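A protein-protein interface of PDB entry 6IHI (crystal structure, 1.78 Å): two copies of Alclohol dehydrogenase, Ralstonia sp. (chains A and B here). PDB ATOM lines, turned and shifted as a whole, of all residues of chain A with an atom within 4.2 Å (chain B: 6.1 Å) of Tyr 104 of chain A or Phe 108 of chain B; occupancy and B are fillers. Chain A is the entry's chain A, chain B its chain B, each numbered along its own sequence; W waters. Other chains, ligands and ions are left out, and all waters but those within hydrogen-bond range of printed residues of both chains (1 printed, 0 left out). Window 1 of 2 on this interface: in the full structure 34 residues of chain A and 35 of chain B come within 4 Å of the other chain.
Among the printed residues, merely in contact across the chains: Pro 101 of chain A with Arg 113 of chain B (3.4 Å), Phe 108 of chain A with Tyr 104 of chain B (3.5 Å), Tyr 104 of chain A with Arg 113 of chain B (3.6 Å), Tyr 104 of chain A with Phe 108 of chain B (3.6 Å), Pro 101 of chain A with Phe 117 of chain B (3.6 Å), Tyr 104 of chain A with Ile 116 of chain B (3.7 Å), Tyr 104 of chain A with Val 112 of chain B (3.7 Å), Phe 108 of chain A with Val 112 of chain B (3.8 Å), Phe 108 of chain A with Phe 108 of chain B (3.8 Å), Val 112 of chain A with Tyr 104 of chain B (3.8 Å), Val 112 of chain A with Phe 108 of chain B (3.8 Å) and Thr 100 of chain A with Phe 117 of chain B (3.9 Å).
OG1 of Thr 100 of chain A lies within hydrogen-bond range of N of His 103 of chain A (2.9 Å). O of Phe 108 of chain B is in hydrogen-bond range of N of Arg 113 of chain B.
Tyr 104 of chain A touches Phe 108 of chain B, and with the chains exchanged Phe 108 of chain A touches Tyr 104 of chain B. Tyr 104 of chain A touches Val 112 of chain B, and with the chains exchanged Val 112 of chain A touches Tyr 104 of chain B. Phe 108 of chain B touches its own counterpart, Phe 108 of chain A. Phe 108 of chain A touches Val 112 of chain B, and with the chains exchanged Val 112 of chain A touches Phe 108 of chain B. 7 positions are printed for both chains. Of the 13 pairs that touch across the chains among the printed residues, 7 have their exchanged pair printed and touching as well.
Printed residues of chain B that touch a printed residue of chain A: Tyr 104, Phe 108, Val 112, Arg 113, Ile 116 and Phe 117. Hydrophobic or aromatic side chains of chain B that line the printed part of chain A: Tyr 104, Phe 108, Val 112, Ile 116 and Phe 117. Hydrophobic or aromatic side chains of chain A within 4 Å of the printed part of chain B: Pro 101, Tyr 104, Phe 108 and Val 112. Among the printed residues, 13 pairs touch across the chains.
OD2 of Asp 105 of chain A lies within salt-bridge range of NH2 of Arg 113 of chain B.
Of the printed residues of chain B, Tyr 104 of chain A touches Phe 108, Val 112, Arg 113 and Ile 116. Phe 108 of chain B touches three residues of chain A. Printed residues of chain B within 4 Å of Val 112 of chain A: Tyr 104 and Phe 108. Printed residues of chain B within 4 Å of Thr 100 of chain A: Phe 117 (3.9 Å). Of the printed residues of chain B, Asp 105 of chain A touches Arg 113. Of the printed residues of chain B, Phe 108 of chain A touches Tyr 104 (3.5 Å), Phe 108 (3.8 Å) and Val 112 (3.8 Å). Of the printed residues of chain A, Val 112 of chain B touches Tyr 104 (3.7 Å) and Phe 108 (3.8 Å). Ala 152 of chain B touches none of the printed residues of chain A. Tyr 150 of chain B touches none of the printed residues of chain A. The nearest printed residue of chain A that does not touch Phe 108 of chain B is Asp 105 of chain A (8.1 Å). The nearest printed residue of chain A that does not touch Arg 113 of chain B is Glu 102 of chain A (5.1 Å).
Water W1 bridges the side-chain hydroxyl of Tyr 104 of chain B (2.9 Å) and the side-chain hydroxyl of Tyr 104 of chain A (2.9 Å).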
ATOM      1  N   THR A 100       5.630   9.343 -15.992  1.00  0.00           N
ATOM      2  CA  THR A 100       6.152  10.293 -15.026  1.00  0.00           C
ATOM      3  C   THR A 100       7.454  10.899 -15.533  1.00  0.00           C
ATOM      4  O   THR A 100       8.119  10.322 -16.401  1.00  0.00           O
ATOM      5  CB  THR A 100       6.417   9.606 -13.679  1.00  0.00           C
ATOM      6  OG1 THR A 100       7.461   8.637 -13.847  1.00  0.00           O
ATOM      7  CG2 THR A 100       5.164   8.915 -13.173  1.00  0.00           C
ATOM      8  N   PRO A 101       7.849  12.069 -15.019  1.00  0.00           N
ATOM      9  CA  PRO A 101       9.163  12.613 -15.395  1.00  0.00           C
ATOM     10  C   PRO A 101      10.298  11.651 -15.099  1.00  0.00           C
ATOM     11  O   PRO A 101      11.272  11.577 -15.860  1.00  0.00           O
ATOM     12  CB  PRO A 101       9.263  13.892 -14.552  1.00  0.00           C
ATOM     13  CG  PRO A 101       7.842  14.291 -14.307  1.00  0.00           C
ATOM     14  CD  PRO A 101       7.083  13.002 -14.171  1.00  0.00           C
ATOM     15  N   GLU A 102      10.189  10.911 -13.995  1.00  0.00           N
ATOM     16  CA  GLU A 102      11.220   9.952 -13.620  1.00  0.00           C
ATOM     17  C   GLU A 102      11.291   8.792 -14.609  1.00  0.00           C
ATOM     18  O   GLU A 102      12.386   8.347 -14.972  1.00  0.00           O
ATOM     19  CB  GLU A 102      10.953   9.451 -12.200  1.00  0.00           C
ATOM     20  CG  GLU A 102      11.116  10.525 -11.123  1.00  0.00           C
ATOM     21  CD  GLU A 102       9.914  11.464 -11.001  1.00  0.00           C
ATOM     22  OE1 GLU A 102       8.864  11.205 -11.631  1.00  0.00           O
ATOM     23  OE2 GLU A 102      10.023  12.473 -10.270  1.00  0.00           O
ATOM     24  N   HIS A 103      10.135   8.276 -15.039  1.00  0.00           N
ATOM     25  CA  HIS A 103      10.117   7.219 -16.048  1.00  0.00           C
ATOM     26  C   HIS A 103      10.734   7.697 -17.356  1.00  0.00           C
ATOM     27  O   HIS A 103      11.551   6.996 -17.964  1.00  0.00           O
ATOM     28  CB  HIS A 103       8.687   6.732 -16.279  1.00  0.00           C
ATOM     29  CG  HIS A 103       8.511   5.959 -17.548  1.00  0.00           C
ATOM     30  ND1 HIS A 103       8.906   4.645 -17.685  1.00  0.00           N
ATOM     31  CD2 HIS A 103       7.993   6.323 -18.747  1.00  0.00           C
ATOM     32  CE1 HIS A 103       8.633   4.231 -18.911  1.00  0.00           C
ATOM     33  NE2 HIS A 103       8.076   5.229 -19.574  1.00  0.00           N
ATOM     34  N   TYR A 104      10.340   8.890 -17.813  1.00  0.00           N
ATOM     35  CA  TYR A 104      10.927   9.446 -19.026  1.00  0.00           C
ATOM     36  C   TYR A 104      12.438   9.577 -18.885  1.00  0.00           C
ATOM     37  O   TYR A 104      13.198   9.164 -19.770  1.00  0.00           O
ATOM     38  CB  TYR A 104      10.300  10.809 -19.345  1.00  0.00           C
ATOM     39  CG  TYR A 104      11.045  11.557 -20.432  1.00  0.00           C
ATOM     40  CD1 TYR A 104      12.115  12.391 -20.126  1.00  0.00           C
ATOM     41  CD2 TYR A 104      10.688  11.415 -21.769  1.00  0.00           C
ATOM     42  CE1 TYR A 104      12.813  13.055 -21.113  1.00  0.00           C
ATOM     43  CE2 TYR A 104      11.377  12.086 -22.763  1.00  0.00           C
ATOM     44  CZ  TYR A 104      12.436  12.901 -22.430  1.00  0.00           C
ATOM     45  OH  TYR A 104      13.130  13.568 -23.415  1.00  0.00           O
ATOM     46  N   ASP A 105      12.892  10.151 -17.770  1.00  0.00           N
ATOM     47  CA  ASP A 105      14.318  10.400 -17.594  1.00  0.00           C
ATOM     48  C   ASP A 105      15.111   9.099 -17.565  1.00  0.00           C
ATOM     49  O   ASP A 105      16.174   9.009 -18.184  1.00  0.00           O
ATOM     50  CB  ASP A 105      14.555  11.220 -16.326  1.00  0.00           C
ATOM     51  CG  ASP A 105      14.106  12.666 -16.476  1.00  0.00           C
ATOM     52  OD1 ASP A 105      14.120  13.186 -17.612  1.00  0.00           O
ATOM     53  OD2 ASP A 105      13.738  13.284 -15.458  1.00  0.00           O
ATOM     54  N   ARG A 106      14.604   8.073 -16.875  1.00  0.00           N
ATOM     55  CA  ARG A 106      15.310   6.793 -16.838  1.00  0.00           C
ATOM     56  C   ARG A 106      15.458   6.206 -18.236  1.00  0.00           C
ATOM     57  O   ARG A 106      16.528   5.701 -18.598  1.00  0.00           O
ATOM     58  CB  ARG A 106      14.571   5.796 -15.944  1.00  0.00           C
ATOM     59  CG  ARG A 106      14.680   6.045 -14.451  1.00  0.00           C
ATOM     60  CD  ARG A 106      14.178   4.837 -13.670  1.00  0.00           C
ATOM     61  NE  ARG A 106      12.796   4.493 -14.000  1.00  0.00           N
ATOM     62  CZ  ARG A 106      11.728   5.020 -13.406  1.00  0.00           C
ATOM     63  NH1 ARG A 106      11.875   5.930 -12.449  1.00  0.00           N
ATOM     64  NH2 ARG A 106      10.510   4.645 -13.774  1.00  0.00           N
ATOM     65  N   THR A 107      14.395   6.279 -19.037  1.00  0.00           N
ATOM     66  CA  THR A 107      14.424   5.691 -20.373  1.00  0.00           C
ATOM     67  C   THR A 107      15.397   6.423 -21.289  1.00  0.00           C
ATOM     68  O   THR A 107      16.250   5.796 -21.930  1.00  0.00           O
ATOM     69  CB  THR A 107      13.016   5.691 -20.969  1.00  0.00           C
ATOM     70  OG1 THR A 107      12.154   4.879 -20.159  1.00  0.00           O
ATOM     71  CG2 THR A 107      13.037   5.139 -22.391  1.00  0.00           C
ATOM     72  N   PHE A 108      15.294   7.751 -21.369  1.00  0.00           N
ATOM     73  CA  PHE A 108      16.174   8.464 -22.286  1.00  0.00           C
ATOM     74  C   PHE A 108      17.600   8.575 -21.750  1.00  0.00           C
ATOM     75  O   PHE A 108      18.545   8.659 -22.543  1.00  0.00           O
ATOM     76  CB  PHE A 108      15.601   9.842 -22.614  1.00  0.00           C
ATOM     77  CG  PHE A 108      14.563   9.804 -23.700  1.00  0.00           C
ATOM     78  CD1 PHE A 108      13.317   9.249 -23.466  1.00  0.00           C
ATOM     79  CD2 PHE A 108      14.871  10.241 -24.977  1.00  0.00           C
ATOM     80  CE1 PHE A 108      12.363   9.188 -24.476  1.00  0.00           C
ATOM     81  CE2 PHE A 108      13.931  10.176 -25.995  1.00  0.00           C
ATOM     82  CZ  PHE A 108      12.672   9.649 -25.739  1.00  0.00           C
ATOM     83  N   VAL A 112      19.477   7.016 -24.810  1.00  0.00           N
ATOM     84  CA  VAL A 112      19.879   8.086 -25.714  1.00  0.00           C
ATOM     85  C   VAL A 112      21.055   8.874 -25.146  1.00  0.00           C
ATOM     86  O   VAL A 112      22.100   8.991 -25.793  1.00  0.00           O
ATOM     87  CB  VAL A 112      18.694   9.020 -26.027  1.00  0.00           C
ATOM     88  CG1 VAL A 112      19.104  10.061 -27.045  1.00  0.00           C
ATOM     89  CG2 VAL A 112      17.506   8.213 -26.539  1.00  0.00           C
ATOM     90  N   HIS B 103      23.240  21.045 -23.677  1.00  0.00           N
ATOM     91  CA  HIS B 103      22.704  21.072 -25.034  1.00  0.00           C
ATOM     92  C   HIS B 103      21.741  19.916 -25.265  1.00  0.00           C
ATOM     93  O   HIS B 103      20.665  20.096 -25.847  1.00  0.00           O
ATOM     94  CB  HIS B 103      23.842  21.024 -26.050  1.00  0.00           C
ATOM     95  CG  HIS B 103      23.402  20.598 -27.415  1.00  0.00           C
ATOM     96  ND1 HIS B 103      22.729  21.440 -28.275  1.00  0.00           N
ATOM     97  CD2 HIS B 103      23.525  19.416 -28.064  1.00  0.00           C
ATOM     98  CE1 HIS B 103      22.465  20.797 -29.399  1.00  0.00           C
ATOM     99  NE2 HIS B 103      22.935  19.568 -29.297  1.00  0.00           N
ATOM    100  N   TYR B 104      22.127  18.712 -24.832  1.00  0.00           N
ATOM    101  CA  TYR B 104      21.239  17.561 -24.957  1.00  0.00           C
ATOM    102  C   TYR B 104      19.918  17.821 -24.251  1.00  0.00           C
ATOM    103  O   TYR B 104      18.843  17.582 -24.808  1.00  0.00           O
ATOM    104  CB  TYR B 104      21.912  16.311 -24.380  1.00  0.00           C
ATOM    105  CG  TYR B 104      20.956  15.153 -24.194  1.00  0.00           C
ATOM    106  CD1 TYR B 104      20.665  14.295 -25.248  1.00  0.00           C
ATOM    107  CD2 TYR B 104      20.335  14.927 -22.972  1.00  0.00           C
ATOM    108  CE1 TYR B 104      19.786  13.244 -25.089  1.00  0.00           C
ATOM    109  CE2 TYR B 104      19.455  13.883 -22.803  1.00  0.00           C
ATOM    110  CZ  TYR B 104      19.185  13.044 -23.864  1.00  0.00           C
ATOM    111  OH  TYR B 104      18.313  11.997 -23.702  1.00  0.00           O
ATOM    112  N   ASP B 105      19.984  18.313 -23.013  1.00  0.00           N
ATOM    113  CA  ASP B 105      18.774  18.521 -22.230  1.00  0.00           C
ATOM    114  C   ASP B 105      17.876  19.574 -22.865  1.00  0.00           C
ATOM    115  O   ASP B 105      16.659  19.388 -22.943  1.00  0.00           O
ATOM    116  CB  ASP B 105      19.138  18.910 -20.800  1.00  0.00           C
ATOM    117  CG  ASP B 105      19.634  17.734 -19.992  1.00  0.00           C
ATOM    118  OD1 ASP B 105      19.238  16.588 -20.300  1.00  0.00           O
ATOM    119  OD2 ASP B 105      20.419  17.952 -19.046  1.00  0.00           O
ATOM    120  N   ARG B 106      18.458  20.673 -23.354  1.00  0.00           N
ATOM    121  CA  ARG B 106      17.644  21.713 -23.976  1.00  0.00           C
ATOM    122  C   ARG B 106      16.879  21.166 -25.171  1.00  0.00           C
ATOM    123  O   ARG B 106      15.694  21.470 -25.355  1.00  0.00           O
ATOM    124  CB  ARG B 106      18.522  22.882 -24.421  1.00  0.00           C
ATOM    125  CG  ARG B 106      19.015  23.780 -23.301  1.00  0.00           C
ATOM    126  CD  ARG B 106      19.575  25.080 -23.861  1.00  0.00           C
ATOM    127  NE  ARG B 106      20.780  24.872 -24.656  1.00  0.00           N
ATOM    128  CZ  ARG B 106      22.007  24.799 -24.147  1.00  0.00           C
ATOM    129  NH1 ARG B 106      22.191  24.909 -22.837  1.00  0.00           N
ATOM    130  NH2 ARG B 106      23.050  24.612 -24.945  1.00  0.00           N
ATOM    131  N   THR B 107      17.544  20.357 -25.994  1.00  0.00           N
ATOM    132  CA  THR B 107      16.904  19.820 -27.191  1.00  0.00           C
ATOM    133  C   THR B 107      15.805  18.827 -26.834  1.00  0.00           C
ATOM    134  O   THR B 107      14.677  18.935 -27.326  1.00  0.00           O
ATOM    135  CB  THR B 107      17.960  19.179 -28.094  1.00  0.00           C
ATOM    136  OG1 THR B 107      18.891  20.184 -28.519  1.00  0.00           O
ATOM    137  CG2 THR B 107      17.310  18.559 -29.317  1.00  0.00           C
ATOM    138  N   PHE B 108      16.106  17.854 -25.972  1.00  0.00           N
ATOM    139  CA  PHE B 108      15.093  16.849 -25.677  1.00  0.00           C
ATOM    140  C   PHE B 108      14.015  17.346 -24.719  1.00  0.00           C
ATOM    141  O   PHE B 108      12.881  16.858 -24.785  1.00  0.00           O
ATOM    142  CB  PHE B 108      15.752  15.568 -25.159  1.00  0.00           C
ATOM    143  CG  PHE B 108      16.296  14.694 -26.260  1.00  0.00           C
ATOM    144  CD1 PHE B 108      17.446  15.046 -26.943  1.00  0.00           C
ATOM    145  CD2 PHE B 108      15.594  13.568 -26.673  1.00  0.00           C
ATOM    146  CE1 PHE B 108      17.929  14.260 -27.972  1.00  0.00           C
ATOM    147  CE2 PHE B 108      16.067  12.785 -27.707  1.00  0.00           C
ATOM    148  CZ  PHE B 108      17.233  13.129 -28.358  1.00  0.00           C
ATOM    149  N   ASP B 109      14.315  18.316 -23.845  1.00  0.00           N
ATOM    150  CA  ASP B 109      13.278  18.812 -22.940  1.00  0.00           C
ATOM    151  C   ASP B 109      12.141  19.481 -23.706  1.00  0.00           C
ATOM    152  O   ASP B 109      10.966  19.291 -23.374  1.00  0.00           O
ATOM    153  CB  ASP B 109      13.850  19.799 -21.922  1.00  0.00           C
ATOM    154  CG  ASP B 109      14.661  19.117 -20.829  1.00  0.00           C
ATOM    155  OD1 ASP B 109      14.661  17.869 -20.761  1.00  0.00           O
ATOM    156  OD2 ASP B 109      15.288  19.841 -20.028  1.00  0.00           O
ATOM    157  N   VAL B 110      12.465  20.284 -24.717  1.00  0.00           N
ATOM    158  CA  VAL B 110      11.401  20.984 -25.430  1.00  0.00           C
ATOM    159  C   VAL B 110      10.809  20.102 -26.524  1.00  0.00           C
ATOM    160  O   VAL B 110       9.593  20.095 -26.738  1.00  0.00           O
ATOM    161  CB  VAL B 110      11.898  22.337 -25.980  1.00  0.00           C
ATOM    162  CG1 VAL B 110      12.998  22.159 -27.005  1.00  0.00           C
ATOM    163  CG2 VAL B 110      10.728  23.128 -26.572  1.00  0.00           C
ATOM    164  N   ASN B 111      11.643  19.340 -27.231  1.00  0.00           N
ATOM    165  CA  ASN B 111      11.147  18.609 -28.395  1.00  0.00           C
ATOM    166  C   ASN B 111      10.456  17.303 -28.022  1.00  0.00           C
ATOM    167  O   ASN B 111       9.538  16.870 -28.731  1.00  0.00           O
ATOM    168  CB  ASN B 111      12.297  18.326 -29.365  1.00  0.00           C
ATOM    169  CG  ASN B 111      12.700  19.550 -30.155  1.00  0.00           C
ATOM    170  OD1 ASN B 111      11.929  20.059 -30.970  1.00  0.00           O
ATOM    171  ND2 ASN B 111      13.908  20.043 -29.905  1.00  0.00           N
ATOM    172  N   VAL B 112      10.878  16.647 -26.942  1.00  0.00           N
ATOM    173  CA  VAL B 112      10.336  15.331 -26.625  1.00  0.00           C
ATOM    174  C   VAL B 112       9.631  15.351 -25.277  1.00  0.00           C
ATOM    175  O   VAL B 112       8.442  15.032 -25.180  1.00  0.00           O
ATOM    176  CB  VAL B 112      11.438  14.259 -26.642  1.00  0.00           C
ATOM    177  CG1 VAL B 112      10.834  12.886 -26.405  1.00  0.00           C
ATOM    178  CG2 VAL B 112      12.186  14.295 -27.969  1.00  0.00           C
ATOM    179  N   ARG B 113      10.373  15.697 -24.225  1.00  0.00           N
ATOM    180  CA  ARG B 113       9.809  15.694 -22.879  1.00  0.00           C
ATOM    181  C   ARG B 113       8.591  16.605 -22.788  1.00  0.00           C
ATOM    182  O   ARG B 113       7.510  16.175 -22.367  1.00  0.00           O
ATOM    183  CB  ARG B 113      10.883  16.114 -21.875  1.00  0.00           C
ATOM    184  CG  ARG B 113      10.573  15.751 -20.437  1.00  0.00           C
ATOM    185  CD  ARG B 113      11.522  16.480 -19.496  1.00  0.00           C
ATOM    186  NE  ARG B 113      11.886  15.665 -18.341  1.00  0.00           N
ATOM    187  CZ  ARG B 113      11.647  16.022 -17.083  1.00  0.00           C
ATOM    188  NH1 ARG B 113      11.046  17.175 -16.827  1.00  0.00           N
ATOM    189  NH2 ARG B 113      12.007  15.230 -16.084  1.00  0.00           N
ATOM    190  N   GLY B 114       8.752  17.870 -23.180  1.00  0.00           N
ATOM    191  CA  GLY B 114       7.638  18.803 -23.137  1.00  0.00           C
ATOM    192  C   GLY B 114       6.497  18.388 -24.041  1.00  0.00           C
ATOM    193  O   GLY B 114       5.332  18.651 -23.737  1.00  0.00           O
ATOM    194  N   ILE B 116       5.615  15.195 -24.798  1.00  0.00           N
ATOM    195  CA  ILE B 116       4.914  14.113 -24.107  1.00  0.00           C
ATOM    196  C   ILE B 116       3.939  14.676 -23.077  1.00  0.00           C
ATOM    197  O   ILE B 116       2.782  14.250 -22.993  1.00  0.00           O
ATOM    198  CB  ILE B 116       5.928  13.148 -23.462  1.00  0.00           C
ATOM    199  CG1 ILE B 116       6.606  12.306 -24.543  1.00  0.00           C
ATOM    200  CG2 ILE B 116       5.242  12.253 -22.441  1.00  0.00           C
ATOM    201  CD1 ILE B 116       7.812  11.496 -24.061  1.00  0.00           C
ATOM    202  N   PHE B 117       4.388  15.640 -22.271  1.00  0.00           N
ATOM    203  CA  PHE B 117       3.498  16.129 -21.223  1.00  0.00           C
ATOM    204  C   PHE B 117       2.462  17.107 -21.759  1.00  0.00           C
ATOM    205  O   PHE B 117       1.371  17.211 -21.187  1.00  0.00           O
ATOM    206  CB  PHE B 117       4.318  16.735 -20.086  1.00  0.00           C
ATOM    207  CG  PHE B 117       5.093  15.703 -19.325  1.00  0.00           C
ATOM    208  CD1 PHE B 117       4.432  14.787 -18.523  1.00  0.00           C
ATOM    209  CD2 PHE B 117       6.467  15.605 -19.459  1.00  0.00           C
ATOM    210  CE1 PHE B 117       5.134  13.807 -17.842  1.00  0.00           C
ATOM    211  CE2 PHE B 117       7.176  14.628 -18.781  1.00  0.00           C
ATOM    212  CZ  PHE B 117       6.508  13.732 -17.970  1.00  0.00           C
ATOM    213  N   ASP B 148      22.766  16.541 -34.514  1.00  0.00           N
ATOM    214  CA  ASP B 148      22.679  15.257 -33.816  1.00  0.00           C
ATOM    215  C   ASP B 148      21.453  15.158 -32.918  1.00  0.00           C
ATOM    216  O   ASP B 148      20.616  14.266 -33.090  1.00  0.00           O
ATOM    217  CB  ASP B 148      23.933  15.004 -32.968  1.00  0.00           C
ATOM    218  CG  ASP B 148      25.200  15.133 -33.746  1.00  0.00           C
ATOM    219  OD1 ASP B 148      25.324  16.097 -34.521  1.00  0.00           O
ATOM    220  OD2 ASP B 148      26.075  14.248 -33.593  1.00  0.00           O
ATOM    221  N   THR B 149      21.341  16.048 -31.928  1.00  0.00           N
ATOM    222  CA  THR B 149      20.259  15.899 -30.962  1.00  0.00           C
ATOM    223  C   THR B 149      18.918  16.310 -31.561  1.00  0.00           C
ATOM    224  O   THR B 149      17.895  15.672 -31.283  1.00  0.00           O
ATOM    225  CB  THR B 149      20.556  16.695 -29.688  1.00  0.00           C
ATOM    226  OG1 THR B 149      20.648  18.091 -29.998  1.00  0.00           O
ATOM    227  CG2 THR B 149      21.882  16.221 -29.059  1.00  0.00           C
ATOM    228  N   TYR B 150      18.901  17.353 -32.394  1.00  0.00           N
ATOM    229  CA  TYR B 150      17.641  17.809 -32.981  1.00  0.00           C
ATOM    230  C   TYR B 150      17.026  16.729 -33.857  1.00  0.00           C
ATOM    231  O   TYR B 150      15.832  16.423 -33.743  1.00  0.00           O
ATOM    232  CB  TYR B 150      17.858  19.087 -33.796  1.00  0.00           C
ATOM    233  CG  TYR B 150      16.588  19.583 -34.462  1.00  0.00           C
ATOM    234  CD1 TYR B 150      15.632  20.285 -33.738  1.00  0.00           C
ATOM    235  CD2 TYR B 150      16.337  19.333 -35.806  1.00  0.00           C
ATOM    236  CE1 TYR B 150      14.460  20.737 -34.338  1.00  0.00           C
ATOM    237  CE2 TYR B 150      15.163  19.785 -36.419  1.00  0.00           C
ATOM    238  CZ  TYR B 150      14.233  20.481 -35.675  1.00  0.00           C
ATOM    239  OH  TYR B 150      13.068  20.929 -36.266  1.00  0.00           O
ATOM    240  N   ALA B 152      17.623  13.473 -33.815  1.00  0.00           N
ATOM    241  CA  ALA B 152      17.209  12.358 -32.972  1.00  0.00           C
ATOM    242  C   ALA B 152      15.925  12.681 -32.218  1.00  0.00           C
ATOM    243  O   ALA B 152      15.040  11.827 -32.091  1.00  0.00           O
ATOM    244  CB  ALA B 152      18.332  11.989 -32.001  1.00  0.00           C
ATOM    245  N   ALA B 153      15.802  13.910 -31.711  1.00  0.00           N
ATOM    246  CA  ALA B 153      14.587  14.299 -31.004  1.00  0.00           C
ATOM    247  C   ALA B 153      13.377  14.272 -31.928  1.00  0.00           C
ATOM    248  O   ALA B 153      12.299  13.809 -31.541  1.00  0.00           O
ATOM    249  CB  ALA B 153      14.755  15.693 -30.398  1.00  0.00           C
ATOM    250  N   ALA B 156      12.211  10.873 -32.470  1.00  0.00           N
ATOM    251  CA  ALA B 156      11.412  10.431 -31.333  1.00  0.00           C
ATOM    252  C   ALA B 156       9.979  10.934 -31.442  1.00  0.00           C
ATOM    253  O   ALA B 156       9.033  10.223 -31.086  1.00  0.00           O
ATOM    254  CB  ALA B 156      12.041  10.902 -30.020  1.00  0.00           C
HETATM  255  O   HOH W   1      15.917  13.239 -22.638  1.00  0.00           O
